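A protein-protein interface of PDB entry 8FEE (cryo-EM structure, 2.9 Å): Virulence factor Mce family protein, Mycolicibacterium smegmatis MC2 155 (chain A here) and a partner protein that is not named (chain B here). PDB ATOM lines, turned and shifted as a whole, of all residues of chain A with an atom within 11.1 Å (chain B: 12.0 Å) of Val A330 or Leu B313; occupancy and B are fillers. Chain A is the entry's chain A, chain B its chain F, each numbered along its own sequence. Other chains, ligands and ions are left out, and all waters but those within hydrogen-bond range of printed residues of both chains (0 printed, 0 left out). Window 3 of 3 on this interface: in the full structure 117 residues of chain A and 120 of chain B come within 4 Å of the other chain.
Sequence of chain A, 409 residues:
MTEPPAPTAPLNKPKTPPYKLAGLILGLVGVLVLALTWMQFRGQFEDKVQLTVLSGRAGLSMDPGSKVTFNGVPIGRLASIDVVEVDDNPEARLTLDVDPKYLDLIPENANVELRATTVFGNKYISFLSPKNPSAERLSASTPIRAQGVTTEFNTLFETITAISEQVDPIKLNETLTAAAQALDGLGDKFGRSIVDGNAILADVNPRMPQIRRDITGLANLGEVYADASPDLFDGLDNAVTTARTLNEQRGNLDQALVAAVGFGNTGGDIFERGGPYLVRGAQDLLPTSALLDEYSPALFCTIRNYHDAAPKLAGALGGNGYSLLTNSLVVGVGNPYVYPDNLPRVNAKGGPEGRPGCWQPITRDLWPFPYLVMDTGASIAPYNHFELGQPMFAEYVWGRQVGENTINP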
ATOM      1  N   THR A 326      34.696  23.959  12.221  1.00  0.00           N
ATOM      2  CA  THR A 326      33.279  23.952  12.550  1.00  0.00           C
ATOM      3  C   THR A 326      33.026  24.765  13.810  1.00  0.00           C
ATOM      4  O   THR A 326      33.893  24.889  14.677  1.00  0.00           O
ATOM      5  CB  THR A 326      32.749  22.524  12.765  1.00  0.00           C
ATOM      6  OG1 THR A 326      33.596  21.831  13.690  1.00  0.00           O
ATOM      7  CG2 THR A 326      32.694  21.754  11.452  1.00  0.00           C
ATOM      8  N   ASN A 327      31.817  25.318  13.899  1.00  0.00           N
ATOM      9  CA  ASN A 327      31.325  25.980  15.101  1.00  0.00           C
ATOM     10  C   ASN A 327      30.428  25.006  15.851  1.00  0.00           C
ATOM     11  O   ASN A 327      29.436  24.524  15.296  1.00  0.00           O
ATOM     12  CB  ASN A 327      30.553  27.252  14.754  1.00  0.00           C
ATOM     13  CG  ASN A 327      31.406  28.279  14.049  1.00  0.00           C
ATOM     14  OD1 ASN A 327      32.603  28.383  14.304  1.00  0.00           O
ATOM     15  ND2 ASN A 327      30.794  29.047  13.155  1.00  0.00           N
ATOM     16  N   SER A 328      30.762  24.727  17.106  1.00  0.00           N
ATOM     17  CA  SER A 328      29.990  23.796  17.924  1.00  0.00           C
ATOM     18  C   SER A 328      29.328  24.565  19.060  1.00  0.00           C
ATOM     19  O   SER A 328      29.978  24.912  20.048  1.00  0.00           O
ATOM     20  CB  SER A 328      30.881  22.678  18.460  1.00  0.00           C
ATOM     21  OG  SER A 328      31.282  21.804  17.421  1.00  0.00           O
ATOM     22  N   LEU A 329      28.032  24.821  18.924  1.00  0.00           N
ATOM     23  CA  LEU A 329      27.233  25.409  19.989  1.00  0.00           C
ATOM     24  C   LEU A 329      26.304  24.342  20.547  1.00  0.00           C
ATOM     25  O   LEU A 329      25.694  23.588  19.785  1.00  0.00           O
ATOM     26  CB  LEU A 329      26.451  26.627  19.483  1.00  0.00           C
ATOM     27  CG  LEU A 329      25.575  26.537  18.228  1.00  0.00           C
ATOM     28  CD1 LEU A 329      24.150  26.121  18.549  1.00  0.00           C
ATOM     29  CD2 LEU A 329      25.586  27.859  17.473  1.00  0.00           C
ATOM     30  N   VAL A 330      26.229  24.255  21.876  1.00  0.00           N
ATOM     31  CA  VAL A 330      25.439  23.206  22.509  1.00  0.00           C
ATOM     32  C   VAL A 330      23.962  23.412  22.199  1.00  0.00           C
ATOM     33  O   VAL A 330      23.448  24.538  22.240  1.00  0.00           O
ATOM     34  CB  VAL A 330      25.700  23.175  24.025  1.00  0.00           C
ATOM     35  CG1 VAL A 330      27.061  22.562  24.312  1.00  0.00           C
ATOM     36  CG2 VAL A 330      25.618  24.575  24.611  1.00  0.00           C
ATOM     37  N   VAL A 331      23.271  22.319  21.872  1.00  0.00           N
ATOM     38  CA  VAL A 331      21.854  22.358  21.536  1.00  0.00           C
ATOM     39  C   VAL A 331      21.237  21.087  22.112  1.00  0.00           C
ATOM     40  O   VAL A 331      21.938  20.129  22.441  1.00  0.00           O
ATOM     41  CB  VAL A 331      21.627  22.471  20.002  1.00  0.00           C
ATOM     42  CG1 VAL A 331      22.150  21.247  19.271  1.00  0.00           C
ATOM     43  CG2 VAL A 331      20.186  22.802  19.632  1.00  0.00           C
ATOM     44  N   GLY A 332      19.915  21.085  22.237  1.00  0.00           N
ATOM     45  CA  GLY A 332      19.184  19.923  22.719  1.00  0.00           C
ATOM     46  C   GLY A 332      18.647  19.090  21.567  1.00  0.00           C
ATOM     47  O   GLY A 332      18.213  19.626  20.548  1.00  0.00           O
ATOM     48  N   VAL A 333      18.679  17.775  21.747  1.00  0.00           N
ATOM     49  CA  VAL A 333      18.311  16.842  20.698  1.00  0.00           C
ATOM     50  C   VAL A 333      16.853  16.445  20.869  1.00  0.00           C
ATOM     51  O   VAL A 333      16.273  16.537  21.954  1.00  0.00           O
ATOM     52  CB  VAL A 333      19.222  15.595  20.695  1.00  0.00           C
ATOM     53  CG1 VAL A 333      20.532  15.898  19.992  1.00  0.00           C
ATOM     54  CG2 VAL A 333      19.465  15.117  22.119  1.00  0.00           C
ATOM     55  N   GLY A 334      16.251  15.986  19.775  1.00  0.00           N
ATOM     56  CA  GLY A 334      14.877  15.536  19.791  1.00  0.00           C
ATOM     57  C   GLY A 334      14.716  14.145  20.372  1.00  0.00           C
ATOM     58  O   GLY A 334      15.666  13.495  20.809  1.00  0.00           O
ATOM     59  N   ASN A 335      13.469  13.690  20.374  1.00  0.00           N
ATOM     60  CA  ASN A 335      13.137  12.410  20.981  1.00  0.00           C
ATOM     61  C   ASN A 335      13.662  11.263  20.122  1.00  0.00           C
ATOM     62  O   ASN A 335      13.591  11.329  18.890  1.00  0.00           O
ATOM     63  CB  ASN A 335      11.627  12.282  21.160  1.00  0.00           C
ATOM     64  CG  ASN A 335      11.045  13.399  21.995  1.00  0.00           C
ATOM     65  OD1 ASN A 335      10.349  14.273  21.483  1.00  0.00           O
ATOM     66  ND2 ASN A 335      11.326  13.378  23.292  1.00  0.00           N
ATOM     67  N   PRO A 336      14.208  10.213  20.737  1.00  0.00           N
ATOM     68  CA  PRO A 336      14.707   9.077  19.955  1.00  0.00           C
ATOM     69  C   PRO A 336      13.593   8.405  19.167  1.00  0.00           C
ATOM     70  O   PRO A 336      12.426   8.410  19.568  1.00  0.00           O
ATOM     71  CB  PRO A 336      15.278   8.137  21.022  1.00  0.00           C
ATOM     72  CG  PRO A 336      15.594   9.027  22.175  1.00  0.00           C
ATOM     73  CD  PRO A 336      14.540  10.092  22.166  1.00  0.00           C
ATOM     74  N   PHE A 386      10.041  24.840  23.450  1.00  0.00           N
ATOM     75  CA  PHE A 386      10.897  24.128  24.389  1.00  0.00           C
ATOM     76  C   PHE A 386      10.051  23.187  25.237  1.00  0.00           C
ATOM     77  O   PHE A 386       9.143  23.631  25.948  1.00  0.00           O
ATOM     78  CB  PHE A 386      11.652  25.128  25.267  1.00  0.00           C
ATOM     79  CG  PHE A 386      12.497  24.495  26.336  1.00  0.00           C
ATOM     80  CD1 PHE A 386      13.816  24.157  26.083  1.00  0.00           C
ATOM     81  CD2 PHE A 386      11.986  24.273  27.606  1.00  0.00           C
ATOM     82  CE1 PHE A 386      14.599  23.585  27.067  1.00  0.00           C
ATOM     83  CE2 PHE A 386      12.764  23.700  28.593  1.00  0.00           C
ATOM     84  CZ  PHE A 386      14.073  23.358  28.324  1.00  0.00           C
ATOM     85  N   GLU A 387      10.350  21.892  25.162  1.00  0.00           N
ATOM     86  CA  GLU A 387       9.738  20.893  26.026  1.00  0.00           C
ATOM     87  C   GLU A 387      10.797  19.881  26.432  1.00  0.00           C
ATOM     88  O   GLU A 387      11.766  19.653  25.706  1.00  0.00           O
ATOM     89  CB  GLU A 387       8.565  20.171  25.351  1.00  0.00           C
ATOM     90  CG  GLU A 387       7.361  21.053  25.074  1.00  0.00           C
ATOM     91  CD  GLU A 387       6.068  20.272  25.033  1.00  0.00           C
ATOM     92  OE1 GLU A 387       5.999  19.202  25.672  1.00  0.00           O
ATOM     93  OE2 GLU A 387       5.121  20.724  24.359  1.00  0.00           O
ATOM     94  N   LEU A 388      10.605  19.277  27.601  1.00  0.00           N
ATOM     95  CA  LEU A 388      11.542  18.261  28.056  1.00  0.00           C
ATOM     96  C   LEU A 388      11.385  16.987  27.236  1.00  0.00           C
ATOM     97  O   LEU A 388      10.278  16.621  26.834  1.00  0.00           O
ATOM     98  CB  LEU A 388      11.342  17.972  29.547  1.00  0.00           C
ATOM     99  CG  LEU A 388       9.975  17.539  30.087  1.00  0.00           C
ATOM    100  CD1 LEU A 388       9.785  16.023  30.049  1.00  0.00           C
ATOM    101  CD2 LEU A 388       9.779  18.068  31.500  1.00  0.00           C
ATOM    102  N   GLY A 389      12.510  16.329  26.965  1.00  0.00           N
ATOM    103  CA  GLY A 389      12.513  15.085  26.223  1.00  0.00           C
ATOM    104  C   GLY A 389      11.724  14.015  26.946  1.00  0.00           C
ATOM    105  O   GLY A 389      12.039  13.694  28.096  1.00  0.00           O
ATOM    106  N   PRO A 391      11.342  10.641  26.846  1.00  0.00           N
ATOM    107  CA  PRO A 391      12.184   9.670  27.579  1.00  0.00           C
ATOM    108  C   PRO A 391      13.303  10.370  28.343  1.00  0.00           C
ATOM    109  O   PRO A 391      14.493  10.236  28.034  1.00  0.00           O
ATOM    110  CB  PRO A 391      12.709   8.767  26.454  1.00  0.00           C
ATOM    111  CG  PRO A 391      11.863   9.062  25.256  1.00  0.00           C
ATOM    112  CD  PRO A 391      11.502  10.494  25.390  1.00  0.00           C
ATOM    113  N   MET A 392      12.920  11.158  29.355  1.00  0.00           N
ATOM    114  CA  MET A 392      13.902  11.923  30.121  1.00  0.00           C
ATOM    115  C   MET A 392      14.902  11.015  30.825  1.00  0.00           C
ATOM    116  O   MET A 392      16.105  11.302  30.846  1.00  0.00           O
ATOM    117  CB  MET A 392      13.188  12.820  31.132  1.00  0.00           C
ATOM    118  CG  MET A 392      14.081  13.350  32.242  1.00  0.00           C
ATOM    119  SD  MET A 392      13.166  14.257  33.501  1.00  0.00           S
ATOM    120  CE  MET A 392      12.511  15.613  32.531  1.00  0.00           C
ATOM    121  N   TYR A 396      19.118   0.600  31.388  1.00  0.00           N
ATOM    122  CA  TYR A 396      19.527  -0.431  30.444  1.00  0.00           C
ATOM    123  C   TYR A 396      19.853  -1.747  31.143  1.00  0.00           C
ATOM    124  O   TYR A 396      20.669  -2.532  30.654  1.00  0.00           O
ATOM    125  CB  TYR A 396      20.721   0.058  29.628  1.00  0.00           C
ATOM    126  CG  TYR A 396      20.454   1.378  28.944  1.00  0.00           C
ATOM    127  CD1 TYR A 396      19.258   1.608  28.282  1.00  0.00           C
ATOM    128  CD2 TYR A 396      21.384   2.404  28.990  1.00  0.00           C
ATOM    129  CE1 TYR A 396      19.005   2.814  27.666  1.00  0.00           C
ATOM    130  CE2 TYR A 396      21.140   3.615  28.378  1.00  0.00           C
ATOM    131  CZ  TYR A 396      19.948   3.814  27.720  1.00  0.00           C
ATOM    132  OH  TYR A 396      19.703   5.021  27.108  1.00  0.00           O
ATOM    133  N   GLY B 307      31.951  25.834   8.918  1.00  0.00           N
ATOM    134  CA  GLY B 307      30.564  25.420   8.769  1.00  0.00           C
ATOM    135  C   GLY B 307      29.995  24.929  10.090  1.00  0.00           C
ATOM    136  O   GLY B 307      30.673  24.241  10.848  1.00  0.00           O
ATOM    137  N   LEU B 308      28.737  25.277  10.344  1.00  0.00           N
ATOM    138  CA  LEU B 308      28.125  25.002  11.638  1.00  0.00           C
ATOM    139  C   LEU B 308      27.930  23.505  11.861  1.00  0.00           C
ATOM    140  O   LEU B 308      27.511  22.773  10.962  1.00  0.00           O
ATOM    141  CB  LEU B 308      26.785  25.723  11.744  1.00  0.00           C
ATOM    142  CG  LEU B 308      26.833  27.231  11.510  1.00  0.00           C
ATOM    143  CD1 LEU B 308      25.466  27.759  11.123  1.00  0.00           C
ATOM    144  CD2 LEU B 308      27.345  27.932  12.753  1.00  0.00           C
ATOM    145  N   LEU B 309      28.237  23.058  13.081  1.00  0.00           N
ATOM    146  CA  LEU B 309      28.016  21.671  13.490  1.00  0.00           C
ATOM    147  C   LEU B 309      27.860  21.686  15.008  1.00  0.00           C
ATOM    148  O   LEU B 309      28.852  21.791  15.732  1.00  0.00           O
ATOM    149  CB  LEU B 309      29.165  20.772  13.053  1.00  0.00           C
ATOM    150  CG  LEU B 309      29.084  19.253  13.269  1.00  0.00           C
ATOM    151  CD1 LEU B 309      29.931  18.552  12.231  1.00  0.00           C
ATOM    152  CD2 LEU B 309      29.535  18.822  14.659  1.00  0.00           C
ATOM    153  N   HIS B 310      26.624  21.560  15.473  1.00  0.00           N
ATOM    154  CA  HIS B 310      26.305  21.647  16.888  1.00  0.00           C
ATOM    155  C   HIS B 310      26.483  20.302  17.588  1.00  0.00           C
ATOM    156  O   HIS B 310      26.734  19.270  16.964  1.00  0.00           O
ATOM    157  CB  HIS B 310      24.879  22.156  17.060  1.00  0.00           C
ATOM    158  CG  HIS B 310      24.500  23.208  16.069  1.00  0.00           C
ATOM    159  ND1 HIS B 310      25.331  24.260  15.750  1.00  0.00           N
ATOM    160  CD2 HIS B 310      23.390  23.363  15.312  1.00  0.00           C
ATOM    161  CE1 HIS B 310      24.745  25.024  14.848  1.00  0.00           C
ATOM    162  NE2 HIS B 310      23.567  24.501  14.562  1.00  0.00           N
ATOM    163  N   PHE B 311      26.350  20.329  18.911  1.00  0.00           N
ATOM    164  CA  PHE B 311      26.442  19.137  19.738  1.00  0.00           C
ATOM    165  C   PHE B 311      25.137  18.942  20.494  1.00  0.00           C
ATOM    166  O   PHE B 311      24.467  19.909  20.863  1.00  0.00           O
ATOM    167  CB  PHE B 311      27.607  19.228  20.729  1.00  0.00           C
ATOM    168  CG  PHE B 311      28.918  18.771  20.164  1.00  0.00           C
ATOM    169  CD1 PHE B 311      28.960  17.802  19.177  1.00  0.00           C
ATOM    170  CD2 PHE B 311      30.108  19.310  20.621  1.00  0.00           C
ATOM    171  CE1 PHE B 311      30.164  17.377  18.655  1.00  0.00           C
ATOM    172  CE2 PHE B 311      31.315  18.890  20.103  1.00  0.00           C
ATOM    173  CZ  PHE B 311      31.343  17.922  19.118  1.00  0.00           C
ATOM    174  N   GLY B 312      24.800  17.682  20.761  1.00  0.00           N
ATOM    175  CA  GLY B 312      23.559  17.342  21.416  1.00  0.00           C
ATOM    176  C   GLY B 312      23.742  17.028  22.886  1.00  0.00           C
ATOM    177  O   GLY B 312      24.532  16.156  23.253  1.00  0.00           O
ATOM    178  N   LEU B 313      23.003  17.746  23.725  1.00  0.00           N
ATOM    179  CA  LEU B 313      23.039  17.495  25.155  1.00  0.00           C
ATOM    180  C   LEU B 313      22.285  16.209  25.487  1.00  0.00           C
ATOM    181  O   LEU B 313      21.518  15.677  24.680  1.00  0.00           O
ATOM    182  CB  LEU B 313      22.441  18.673  25.922  1.00  0.00           C
ATOM    183  CG  LEU B 313      23.154  20.018  25.754  1.00  0.00           C
ATOM    184  CD1 LEU B 313      22.601  21.043  26.729  1.00  0.00           C
ATOM    185  CD2 LEU B 313      24.655  19.861  25.933  1.00  0.00           C
ATOM    186  N   GLY B 314      22.516  15.707  26.696  1.00  0.00           N
ATOM    187  CA  GLY B 314      21.954  14.436  27.100  1.00  0.00           C
ATOM    188  C   GLY B 314      22.960  13.313  26.968  1.00  0.00           C
ATOM    189  O   GLY B 314      23.667  13.228  25.960  1.00  0.00           O
ATOM    190  N   ILE B 315      23.037  12.444  27.970  1.00  0.00           N
ATOM    191  CA  ILE B 315      24.069  11.415  28.036  1.00  0.00           C
ATOM    192  C   ILE B 315      23.403  10.050  27.928  1.00  0.00           C
ATOM    193  O   ILE B 315      22.507   9.722  28.716  1.00  0.00           O
ATOM    194  CB  ILE B 315      24.902  11.533  29.321  1.00  0.00           C
ATOM    195  CG1 ILE B 315      24.004  11.813  30.529  1.00  0.00           C
ATOM    196  CG2 ILE B 315      25.951  12.623  29.175  1.00  0.00           C
ATOM    197  CD1 ILE B 315      24.760  11.950  31.832  1.00  0.00           C
ATOM    198  N   ASN B 316      23.846   9.263  26.944  1.00  0.00           N
ATOM    199  CA  ASN B 316      23.390   7.886  26.736  1.00  0.00           C
ATOM    200  C   ASN B 316      21.871   7.792  26.609  1.00  0.00           C
ATOM    201  O   ASN B 316      21.231   6.925  27.207  1.00  0.00           O
ATOM    202  CB  ASN B 316      23.895   6.968  27.852  1.00  0.00           C
ATOM    203  CG  ASN B 316      25.242   6.358  27.539  1.00  0.00           C
ATOM    204  OD1 ASN B 316      26.015   6.902  26.753  1.00  0.00           O
ATOM    205  ND2 ASN B 316      25.531   5.216  28.154  1.00  0.00           N
ATOM    206  N   ALA B 317      21.281   8.700  25.815  1.00  0.00           N
ATOM    207  CA  ALA B 317      19.837   8.608  25.592  1.00  0.00           C
ATOM    208  C   ALA B 317      19.507   7.390  24.731  1.00  0.00           C
ATOM    209  O   ALA B 317      18.791   6.496  25.215  1.00  0.00           O
ATOM    210  CB  ALA B 317      19.289   9.945  25.075  1.00  0.00           C
ATOM    211  N   PRO B 318      19.974   7.270  23.483  1.00  0.00           N
ATOM    212  CA  PRO B 318      20.076   5.935  22.897  1.00  0.00           C
ATOM    213  C   PRO B 318      21.475   5.378  23.085  1.00  0.00           C
ATOM    214  O   PRO B 318      22.465   6.010  22.689  1.00  0.00           O
ATOM    215  CB  PRO B 318      19.757   6.171  21.414  1.00  0.00           C
ATOM    216  CG  PRO B 318      20.075   7.602  21.166  1.00  0.00           C
ATOM    217  CD  PRO B 318      20.369   8.277  22.477  1.00  0.00           C
ATOM    218  N   PRO B 319      21.610   4.192  23.667  1.00  0.00           N
ATOM    219  CA  PRO B 319      22.929   3.570  23.750  1.00  0.00           C
ATOM    220  C   PRO B 319      23.283   2.921  22.425  1.00  0.00           C
ATOM    221  O   PRO B 319      22.517   2.097  21.905  1.00  0.00           O
ATOM    222  CB  PRO B 319      22.758   2.526  24.862  1.00  0.00           C
ATOM    223  CG  PRO B 319      21.315   2.175  24.815  1.00  0.00           C
ATOM    224  CD  PRO B 319      20.583   3.422  24.388  1.00  0.00           C
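Among the printed residues, merely in contact across the chains: Thr A326 with Gly B307, Leu A329 with His B310, Tyr A396 with Pro B319, Val A333 with Leu B313, Val A331 with Gly B312, Val A331 with His B310, Val A333 with Gly B312, Asn A327 with Leu B308, Val A330 with Phe B311, Ser A328 with Phe B311, Val A330 with Leu B313 and Thr A326 with Leu B309.
Hydrophobic or aromatic side chains of chain A that line the printed part of chain B: Leu A329, Val A330, Val A331, Val A333 and Tyr A396.
Along chain A the printed residues that touch a printed residue of chain B span positions 326 to 396.
Among the printed residues, 20 pairs touch across the chains.
Of chain A, only Val A330 (3.96 Å), Val A331 (2.9 Å) and Val A333 (3.3 Å) come within 4 Å of Leu B313.
Ser A328 touches two residues of chain B.
Of chain B, only His B310, Phe B311, Gly B312 and Leu B313 come within 4 Å of Val A331.
No residue of chain A comes within 4 Å of Gly B314.
Of the printed residues of chain B, Thr A326 touches Gly B307 and Leu B309.
Printed residues of chain A within 4 Å of Pro B319: Tyr A396 (3.3 Å).
Of the printed residues of chain A, His B310 touches Leu A329 and Val A331.
Gly A334 touches none of the printed residues of chain B.
Pro B318 touches none of the printed residues of chain A.
The nearest residue of chain B that does not touch Val A330 is His B310 (5.4 Å).
The nearest residue of chain A that does not touch Leu B313 is Gly A332 (4.5 Å).
The nearest printed residue of chain A that does not touch Gly B307 is Ser A328 (6.3 Å).
The backbone NH of Asn A327 is in hydrogen-bond range of the backbone carbonyl oxygen of Gly B307 (3.4 Å).
O of Asn A327 sits at hydrogen-bond distance from N of Leu B309 (2.9 Å).
OG of Ser A328 lies within hydrogen-bond range of O of Leu B309, at 3.0 Å.
The backbone carbonyl oxygen (O) of Leu A329 sits at hydrogen-bond distance from the backbone NH (N) of Phe B311, at 3.4 Å.
The backbone NH of Val A331 sits at hydrogen-bond distance from the backbone carbonyl oxygen of Phe B311 (2.9 Å).
N of Leu B313 is in hydrogen-bond range of O of Val A331.
The side-chain hydroxyl (OH) of Tyr A396 lies within hydrogen-bond range of the backbone carbonyl oxygen (O) of Asn B316, at 2.4 Å.
OH of Tyr A396 is in hydrogen-bond range of O of Ala B317.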
